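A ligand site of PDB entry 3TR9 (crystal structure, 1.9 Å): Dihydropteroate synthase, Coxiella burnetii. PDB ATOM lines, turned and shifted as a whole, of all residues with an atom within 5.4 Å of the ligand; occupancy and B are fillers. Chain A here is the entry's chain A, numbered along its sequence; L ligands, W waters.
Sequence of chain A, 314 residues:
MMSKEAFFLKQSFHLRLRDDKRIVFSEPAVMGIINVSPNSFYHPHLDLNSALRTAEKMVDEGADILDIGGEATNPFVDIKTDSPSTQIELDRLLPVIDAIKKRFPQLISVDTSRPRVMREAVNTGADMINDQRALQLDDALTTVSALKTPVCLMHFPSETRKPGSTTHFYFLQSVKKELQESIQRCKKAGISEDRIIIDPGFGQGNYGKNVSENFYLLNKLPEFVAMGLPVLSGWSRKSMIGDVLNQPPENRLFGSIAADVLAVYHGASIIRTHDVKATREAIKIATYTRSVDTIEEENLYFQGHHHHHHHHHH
OD2 of Asp 111 sits at hydrogen-bond distance from N5 of the ligand (2.8 Å). O1 of the ligand lies within hydrogen-bond range of N of Gln 204, 2.9 Å away. OD1 of Asn 130 is in hydrogen-bond range of N3 of the ligand, 2.8 Å away. An oxygen (O2) of the ligand sits at hydrogen-bond distance from the side-chain amino group (NZ) of Lys 238. OG of Ser 239 is in hydrogen-bond range of O1 of the ligand (2.7 Å). The side-chain carboxylate of Asp 199 lies within hydrogen-bond range of a nitrogen (N4) of the ligand. A nitrogen (N5) of the ligand lies close to the guanidinium group of Arg 272, 3.3 Å away. The side-chain hydroxyl of Tyr 207 lies within hydrogen-bond range of a nitrogen (N1) of the ligand (3.2 Å). An oxygen (O3) of the ligand is in hydrogen-bond range of the backbone NH of Ser 239 (2.8 Å). SG of Cys 152 lies within hydrogen-bond range of N3 of the ligand, 3.7 Å away. The side-chain amide nitrogen (NE2) of Gln 132 lies within hydrogen-bond range of a nitrogen (N5) of the ligand, at 3.4 Å.
OE1 of Gln 132 lies within hydrogen-bond range of OH of Tyr 207 (2.6 Å). NZ of Lys 238 sits at hydrogen-bond distance from O of Phe 202, 2.8 Å away. OH of Tyr 207 sits close to SD of Met 154 (3.4 Å). The backbone carbonyl oxygen of Gly 234 is in hydrogen-bond range of the side-chain amino group of Lys 238, at 2.7 Å. N of Arg 272 sits at hydrogen-bond distance from O of Ser 233, at 3.0 Å. The side-chain sulfur (SG) of Cys 152 sits close to the side-chain amide oxygen (OD1) of Asn 130, at 3.8 Å. The side-chain amide nitrogen (ND2) of Asn 130 lies within hydrogen-bond range of the side-chain carboxylate (OD2) of Asp 111 (3.3 Å). The side-chain carboxylate (OD1) of Asp 111 sits at hydrogen-bond distance from the side-chain amide nitrogen (NE2) of Gln 132 (3.0 Å).
SD of Met 154 lies close to N4 of the ligand (3.6 Å). Merely in contact with the ligand: Phe 41, Phe 202, Gly 203, Leu 232 and Gly 234. Hydrophobic or aromatic side chains that line the ligand: Phe 41, Met 154, Tyr 207 and Leu 232. 16 residues have an atom within 4 Å of the ligand: Phe 41, Asp 111, Asn 130, Gln 132, Cys 152, Met 154, Asp 199, Phe 202, Gly 203, Gln 204, Tyr 207, Leu 232, Gly 234, Lys 238, Ser 239 and Arg 272. The nearest printed residue that does not touch the ligand is Met 240 (4.2 Å).
Water W1 lies within hydrogen-bond range of O2 of the ligand (2.7 Å), OD1 of Asp 199 (2.8 Å), N of Phe 202 (3.0 Å) and N of Gly 234 (3.1 Å). Water W3 lies within hydrogen-bond range of O1 of the ligand (2.8 Å) and N of Gly 205 (3.4 Å).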
ATOM      1  N   PHE A  41      11.813  17.000  19.945  1.00  0.00           N
ATOM      2  CA  PHE A  41      11.945  16.471  18.612  1.00  0.00           C
ATOM      3  C   PHE A  41      12.104  14.946  18.579  1.00  0.00           C
ATOM      4  O   PHE A  41      12.733  14.352  19.464  1.00  0.00           O
ATOM      5  CB  PHE A  41      13.109  17.146  17.901  1.00  0.00           C
ATOM      6  CG  PHE A  41      13.339  16.633  16.510  1.00  0.00           C
ATOM      7  CD1 PHE A  41      12.397  16.836  15.511  1.00  0.00           C
ATOM      8  CD2 PHE A  41      14.500  15.951  16.197  1.00  0.00           C
ATOM      9  CE1 PHE A  41      12.611  16.363  14.233  1.00  0.00           C
ATOM     10  CE2 PHE A  41      14.715  15.471  14.912  1.00  0.00           C
ATOM     11  CZ  PHE A  41      13.769  15.674  13.940  1.00  0.00           C
ATOM     12  N   ASP A  67      22.974  13.094  26.298  1.00  0.00           N
ATOM     13  CA  ASP A  67      22.509  14.489  26.357  1.00  0.00           C
ATOM     14  C   ASP A  67      21.034  14.558  26.716  1.00  0.00           C
ATOM     15  O   ASP A  67      20.167  14.143  25.937  1.00  0.00           O
ATOM     16  CB  ASP A  67      22.781  15.206  25.022  1.00  0.00           C
ATOM     17  CG  ASP A  67      22.534  16.715  25.099  1.00  0.00           C
ATOM     18  OD1 ASP A  67      22.877  17.332  26.137  1.00  0.00           O
ATOM     19  OD2 ASP A  67      22.019  17.305  24.123  1.00  0.00           O
ATOM     20  N   ASP A 111      21.156  19.686  28.178  1.00  0.00           N
ATOM     21  CA  ASP A 111      20.794  20.604  27.100  1.00  0.00           C
ATOM     22  C   ASP A 111      19.816  21.645  27.667  1.00  0.00           C
ATOM     23  O   ASP A 111      18.622  21.382  27.773  1.00  0.00           O
ATOM     24  CB  ASP A 111      20.142  19.808  25.967  1.00  0.00           C
ATOM     25  CG  ASP A 111      20.013  20.604  24.677  1.00  0.00           C
ATOM     26  OD1 ASP A 111      20.002  21.841  24.747  1.00  0.00           O
ATOM     27  OD2 ASP A 111      19.919  19.991  23.589  1.00  0.00           O
ATOM     28  N   ASN A 130      25.214  21.695  27.410  1.00  0.00           N
ATOM     29  CA  ASN A 130      25.019  21.892  25.980  1.00  0.00           C
ATOM     30  C   ASN A 130      24.009  23.009  25.764  1.00  0.00           C
ATOM     31  O   ASN A 130      22.824  22.829  26.017  1.00  0.00           O
ATOM     32  CB  ASN A 130      24.536  20.596  25.333  1.00  0.00           C
ATOM     33  CG  ASN A 130      24.131  20.790  23.887  1.00  0.00           C
ATOM     34  OD1 ASN A 130      24.667  21.649  23.184  1.00  0.00           O
ATOM     35  ND2 ASN A 130      23.173  19.988  23.431  1.00  0.00           N
ATOM     36  N   GLN A 132      22.216  25.427  23.134  1.00  0.00           N
ATOM     37  CA  GLN A 132      21.825  25.819  21.793  1.00  0.00           C
ATOM     38  C   GLN A 132      21.904  27.328  21.637  1.00  0.00           C
ATOM     39  O   GLN A 132      22.045  27.842  20.523  1.00  0.00           O
ATOM     40  CB  GLN A 132      20.403  25.361  21.522  1.00  0.00           C
ATOM     41  CG  GLN A 132      20.226  23.847  21.442  1.00  0.00           C
ATOM     42  CD  GLN A 132      18.775  23.457  21.368  1.00  0.00           C
ATOM     43  OE1 GLN A 132      18.091  23.769  20.399  1.00  0.00           O
ATOM     44  NE2 GLN A 132      18.292  22.792  22.410  1.00  0.00           N
ATOM     45  N   CYS A 152      29.139  23.144  25.329  1.00  0.00           N
ATOM     46  CA  CYS A 152      28.987  23.250  23.881  1.00  0.00           C
ATOM     47  C   CYS A 152      28.249  24.527  23.521  1.00  0.00           C
ATOM     48  O   CYS A 152      27.165  24.790  24.031  1.00  0.00           O
ATOM     49  CB  CYS A 152      28.242  22.048  23.299  1.00  0.00           C
ATOM     50  SG  CYS A 152      27.989  22.201  21.495  1.00  0.00           S
ATOM     51  N   MET A 154      26.513  26.528  20.506  1.00  0.00           N
ATOM     52  CA  MET A 154      25.953  26.358  19.182  1.00  0.00           C
ATOM     53  C   MET A 154      25.742  27.717  18.512  1.00  0.00           C
ATOM     54  O   MET A 154      25.618  28.738  19.183  1.00  0.00           O
ATOM     55  CB  MET A 154      24.615  25.635  19.267  1.00  0.00           C
ATOM     56  CG  MET A 154      24.246  24.894  17.982  1.00  0.00           C
ATOM     57  SD  MET A 154      22.449  24.108  18.102  1.00  0.00           S
ATOM     58  CE  MET A 154      21.352  25.713  17.833  1.00  0.00           C
ATOM     59  N   ASP A 199      29.512  24.245  17.631  1.00  0.00           N
ATOM     60  CA  ASP A 199      28.519  23.517  16.843  1.00  0.00           C
ATOM     61  C   ASP A 199      27.849  24.487  15.866  1.00  0.00           C
ATOM     62  O   ASP A 199      27.266  25.478  16.287  1.00  0.00           O
ATOM     63  CB  ASP A 199      27.481  22.939  17.802  1.00  0.00           C
ATOM     64  CG  ASP A 199      26.374  22.181  17.098  1.00  0.00           C
ATOM     65  OD1 ASP A 199      26.148  22.388  15.892  1.00  0.00           O
ATOM     66  OD2 ASP A 199      25.712  21.364  17.770  1.00  0.00           O
ATOM     67  N   GLY A 201      25.170  24.388  14.382  1.00  0.00           N
ATOM     68  CA  GLY A 201      23.726  24.454  14.524  1.00  0.00           C
ATOM     69  C   GLY A 201      22.929  23.941  13.332  1.00  0.00           C
ATOM     70  O   GLY A 201      22.149  24.691  12.721  1.00  0.00           O
ATOM     71  N   PHE A 202      23.111  22.675  12.978  1.00  0.00           N
ATOM     72  CA  PHE A 202      22.390  22.112  11.818  1.00  0.00           C
ATOM     73  C   PHE A 202      20.904  21.985  12.129  1.00  0.00           C
ATOM     74  O   PHE A 202      20.542  21.560  13.220  1.00  0.00           O
ATOM     75  CB  PHE A 202      22.960  20.760  11.439  1.00  0.00           C
ATOM     76  CG  PHE A 202      24.346  20.834  10.842  1.00  0.00           C
ATOM     77  CD1 PHE A 202      25.443  20.369  11.545  1.00  0.00           C
ATOM     78  CD2 PHE A 202      24.537  21.393   9.593  1.00  0.00           C
ATOM     79  CE1 PHE A 202      26.711  20.448  10.995  1.00  0.00           C
ATOM     80  CE2 PHE A 202      25.807  21.487   9.030  1.00  0.00           C
ATOM     81  CZ  PHE A 202      26.894  21.007   9.731  1.00  0.00           C
ATOM     82  N   GLY A 203      20.064  22.372  11.175  1.00  0.00           N
ATOM     83  CA  GLY A 203      18.623  22.339  11.372  1.00  0.00           C
ATOM     84  C   GLY A 203      17.887  23.396  10.580  1.00  0.00           C
ATOM     85  O   GLY A 203      18.496  24.331  10.068  1.00  0.00           O
ATOM     86  N   GLN A 204      16.582  23.249  10.459  1.00  0.00           N
ATOM     87  CA  GLN A 204      15.759  24.289   9.854  1.00  0.00           C
ATOM     88  C   GLN A 204      14.846  24.899  10.922  1.00  0.00           C
ATOM     89  O   GLN A 204      15.217  24.941  12.089  1.00  0.00           O
ATOM     90  CB  GLN A 204      14.970  23.719   8.677  1.00  0.00           C
ATOM     91  CG  GLN A 204      15.892  23.138   7.611  1.00  0.00           C
ATOM     92  CD  GLN A 204      15.164  22.796   6.346  1.00  0.00           C
ATOM     93  OE1 GLN A 204      15.040  23.621   5.450  1.00  0.00           O
ATOM     94  NE2 GLN A 204      14.662  21.568   6.262  1.00  0.00           N
ATOM     95  N   GLY A 205      13.664  25.372  10.536  1.00  0.00           N
ATOM     96  CA  GLY A 205      12.755  25.969  11.505  1.00  0.00           C
ATOM     97  C   GLY A 205      13.417  27.118  12.253  1.00  0.00           C
ATOM     98  O   GLY A 205      13.941  28.053  11.628  1.00  0.00           O
ATOM     99  N   TYR A 207      16.101  27.275  13.625  1.00  0.00           N
ATOM    100  CA  TYR A 207      17.540  27.323  13.441  1.00  0.00           C
ATOM    101  C   TYR A 207      17.938  28.243  12.278  1.00  0.00           C
ATOM    102  O   TYR A 207      19.118  28.403  11.989  1.00  0.00           O
ATOM    103  CB  TYR A 207      18.127  25.925  13.235  1.00  0.00           C
ATOM    104  CG  TYR A 207      18.387  25.172  14.530  1.00  0.00           C
ATOM    105  CD1 TYR A 207      17.667  25.450  15.684  1.00  0.00           C
ATOM    106  CD2 TYR A 207      19.376  24.192  14.595  1.00  0.00           C
ATOM    107  CE1 TYR A 207      17.910  24.762  16.870  1.00  0.00           C
ATOM    108  CE2 TYR A 207      19.630  23.504  15.782  1.00  0.00           C
ATOM    109  CZ  TYR A 207      18.893  23.790  16.912  1.00  0.00           C
ATOM    110  OH  TYR A 207      19.150  23.103  18.072  1.00  0.00           O
ATOM    111  N   LEU A 232      31.031  19.790  17.317  1.00  0.00           N
ATOM    112  CA  LEU A 232      29.907  18.869  17.472  1.00  0.00           C
ATOM    113  C   LEU A 232      28.946  19.068  16.320  1.00  0.00           C
ATOM    114  O   LEU A 232      28.724  20.203  15.880  1.00  0.00           O
ATOM    115  CB  LEU A 232      29.211  19.130  18.814  1.00  0.00           C
ATOM    116  CG  LEU A 232      28.042  18.213  19.213  1.00  0.00           C
ATOM    117  CD1 LEU A 232      27.941  18.110  20.733  1.00  0.00           C
ATOM    118  CD2 LEU A 232      26.718  18.695  18.615  1.00  0.00           C
ATOM    119  N   SER A 233      28.391  17.966  15.809  1.00  0.00           N
ATOM    120  CA  SER A 233      27.445  18.015  14.706  1.00  0.00           C
ATOM    121  C   SER A 233      26.227  17.148  15.020  1.00  0.00           C
ATOM    122  O   SER A 233      26.363  16.024  15.491  1.00  0.00           O
ATOM    123  CB  SER A 233      28.126  17.548  13.408  1.00  0.00           C
ATOM    124  OG  SER A 233      27.194  17.412  12.361  1.00  0.00           O
ATOM    125  N   GLY A 234      25.043  17.697  14.785  1.00  0.00           N
ATOM    126  CA  GLY A 234      23.806  16.972  15.013  1.00  0.00           C
ATOM    127  C   GLY A 234      22.838  17.057  13.843  1.00  0.00           C
ATOM    128  O   GLY A 234      22.090  18.020  13.719  1.00  0.00           O
ATOM    129  N   ARG A 237      18.042  12.566  12.187  1.00  0.00           N
ATOM    130  CA  ARG A 237      16.595  12.497  11.997  1.00  0.00           C
ATOM    131  C   ARG A 237      15.951  13.832  11.608  1.00  0.00           C
ATOM    132  O   ARG A 237      14.729  13.947  11.525  1.00  0.00           O
ATOM    133  CB  ARG A 237      15.909  11.932  13.248  1.00  0.00           C
ATOM    134  CG  ARG A 237      16.415  10.558  13.695  1.00  0.00           C
ATOM    135  CD  ARG A 237      15.951   9.465  12.754  1.00  0.00           C
ATOM    136  NE  ARG A 237      16.352   8.132  13.216  1.00  0.00           N
ATOM    137  CZ  ARG A 237      15.734   7.006  12.874  1.00  0.00           C
ATOM    138  NH1 ARG A 237      14.664   7.042  12.075  1.00  0.00           N
ATOM    139  NH2 ARG A 237      16.171   5.844  13.358  1.00  0.00           N
ATOM    140  N   LYS A 238      16.776  14.843  11.348  1.00  0.00           N
ATOM    141  CA  LYS A 238      16.272  16.192  11.108  1.00  0.00           C
ATOM    142  C   LYS A 238      15.604  16.425   9.740  1.00  0.00           C
ATOM    143  O   LYS A 238      15.741  15.620   8.817  1.00  0.00           O
ATOM    144  CB  LYS A 238      17.354  17.232  11.392  1.00  0.00           C
ATOM    145  CG  LYS A 238      17.718  17.304  12.894  1.00  0.00           C
ATOM    146  CD  LYS A 238      18.780  18.359  13.175  1.00  0.00           C
ATOM    147  CE  LYS A 238      18.980  18.557  14.685  1.00  0.00           C
ATOM    148  NZ  LYS A 238      20.125  19.470  14.961  1.00  0.00           N
ATOM    149  N   SER A 239      14.893  17.543   9.624  1.00  0.00           N
ATOM    150  CA  SER A 239      14.085  17.856   8.452  1.00  0.00           C
ATOM    151  C   SER A 239      14.864  17.935   7.142  1.00  0.00           C
ATOM    152  O   SER A 239      14.288  17.712   6.079  1.00  0.00           O
ATOM    153  CB  SER A 239      13.317  19.167   8.660  1.00  0.00           C
ATOM    154  OG  SER A 239      14.223  20.258   8.756  1.00  0.00           O
ATOM    155  N   MET A 240      16.154  18.295   7.207  1.00  0.00           N
ATOM    156  CA  MET A 240      16.951  18.351   5.992  1.00  0.00           C
ATOM    157  C   MET A 240      16.935  16.982   5.330  1.00  0.00           C
ATOM    158  O   MET A 240      16.835  16.880   4.108  1.00  0.00           O
ATOM    159  CB  MET A 240      18.404  18.760   6.260  1.00  0.00           C
ATOM    160  CG  MET A 240      18.584  20.160   6.830  1.00  0.00           C
ATOM    161  SD  MET A 240      18.323  20.191   8.758  1.00  0.00           S
ATOM    162  CE  MET A 240      19.957  19.274   9.336  1.00  0.00           C
ATOM    163  N   ARG A 252      14.373   8.177   8.462  1.00  0.00           N
ATOM    164  CA  ARG A 252      15.541   8.995   8.147  1.00  0.00           C
ATOM    165  C   ARG A 252      16.869   8.422   8.652  1.00  0.00           C
ATOM    166  O   ARG A 252      17.881   9.112   8.662  1.00  0.00           O
ATOM    167  CB  ARG A 252      15.349  10.405   8.708  1.00  0.00           C
ATOM    168  CG  ARG A 252      14.131  11.101   8.128  1.00  0.00           C
ATOM    169  CD  ARG A 252      13.916  12.490   8.707  1.00  0.00           C
ATOM    170  NE  ARG A 252      12.603  12.990   8.318  1.00  0.00           N
ATOM    171  CZ  ARG A 252      11.992  14.036   8.864  1.00  0.00           C
ATOM    172  NH1 ARG A 252      12.554  14.727   9.848  1.00  0.00           N
ATOM    173  NH2 ARG A 252      10.788  14.404   8.423  1.00  0.00           N
ATOM    174  N   ARG A 272      25.995  14.012  17.740  1.00  0.00           N
ATOM    175  CA  ARG A 272      24.807  13.964  18.579  1.00  0.00           C
ATOM    176  C   ARG A 272      23.696  13.235  17.833  1.00  0.00           C
ATOM    177  O   ARG A 272      23.289  13.657  16.754  1.00  0.00           O
ATOM    178  CB  ARG A 272      24.355  15.397  18.898  1.00  0.00           C
ATOM    179  CG  ARG A 272      23.200  15.503  19.859  1.00  0.00           C
ATOM    180  CD  ARG A 272      22.828  16.973  20.110  1.00  0.00           C
ATOM    181  NE  ARG A 272      21.714  17.102  21.056  1.00  0.00           N
ATOM    182  CZ  ARG A 272      20.431  17.050  20.704  1.00  0.00           C
ATOM    183  NH1 ARG A 272      20.086  16.889  19.432  1.00  0.00           N
ATOM    184  NH2 ARG A 272      19.492  17.167  21.631  1.00  0.00           N
HETATM  185  C1  LIG L   1      22.179  20.381  17.893  1.00  0.00           C
HETATM  186  C2  LIG L   1      21.005  20.257  18.640  1.00  0.00           C
HETATM  187  C3  LIG L   1      21.073  20.442  20.017  1.00  0.00           C
HETATM  188  N1  LIG L   1      19.817  19.984  18.055  1.00  0.00           N
HETATM  189  C4  LIG L   1      23.368  20.817  19.824  1.00  0.00           C
HETATM  190  N2  LIG L   1      22.265  20.708  20.567  1.00  0.00           N
HETATM  191  C5  LIG L   1      18.712  19.875  18.812  1.00  0.00           C
HETATM  192  N3  LIG L   1      24.628  21.111  20.470  1.00  0.00           N
HETATM  193  C6  LIG L   1      18.778  20.059  20.203  1.00  0.00           C
HETATM  194  C7  LIG L   1      14.815  20.148  12.100  1.00  0.00           C
HETATM  195  O1  LIG L   1      15.000  20.963  11.233  1.00  0.00           O
HETATM  196  O2  LIG L   1      22.163  20.212  16.509  1.00  0.00           O
HETATM  197  N4  LIG L   1      23.344  20.661  18.497  1.00  0.00           N
HETATM  198  N5  LIG L   1      19.959  20.325  20.766  1.00  0.00           N
HETATM  199  C8  LIG L   1      17.426  19.596  18.134  1.00  0.00           C
HETATM  200  N6  LIG L   1      16.937  20.789  17.443  1.00  0.00           N
HETATM  201  C9  LIG L   1      16.372  20.664  16.005  1.00  0.00           C
HETATM  202  C10 LIG L   1      15.735  19.481  15.660  1.00  0.00           C
HETATM  203  C11 LIG L   1      16.511  21.691  15.093  1.00  0.00           C
HETATM  204  C12 LIG L   1      15.216  19.325  14.399  1.00  0.00           C
HETATM  205  C13 LIG L   1      15.996  21.528  13.811  1.00  0.00           C
HETATM  206  C14 LIG L   1      15.357  20.352  13.472  1.00  0.00           C
HETATM  207  O3  LIG L   1      14.193  19.042  11.851  1.00  0.00           O
HETATM  208  O   HOH W   1      24.238  20.664  14.859  1.00  0.00           O
HETATM  209  O   HOH W   2      11.550  18.851  12.206  1.00  0.00           O
HETATM  210  O   HOH W   3      12.486  22.299  11.282  1.00  0.00           O
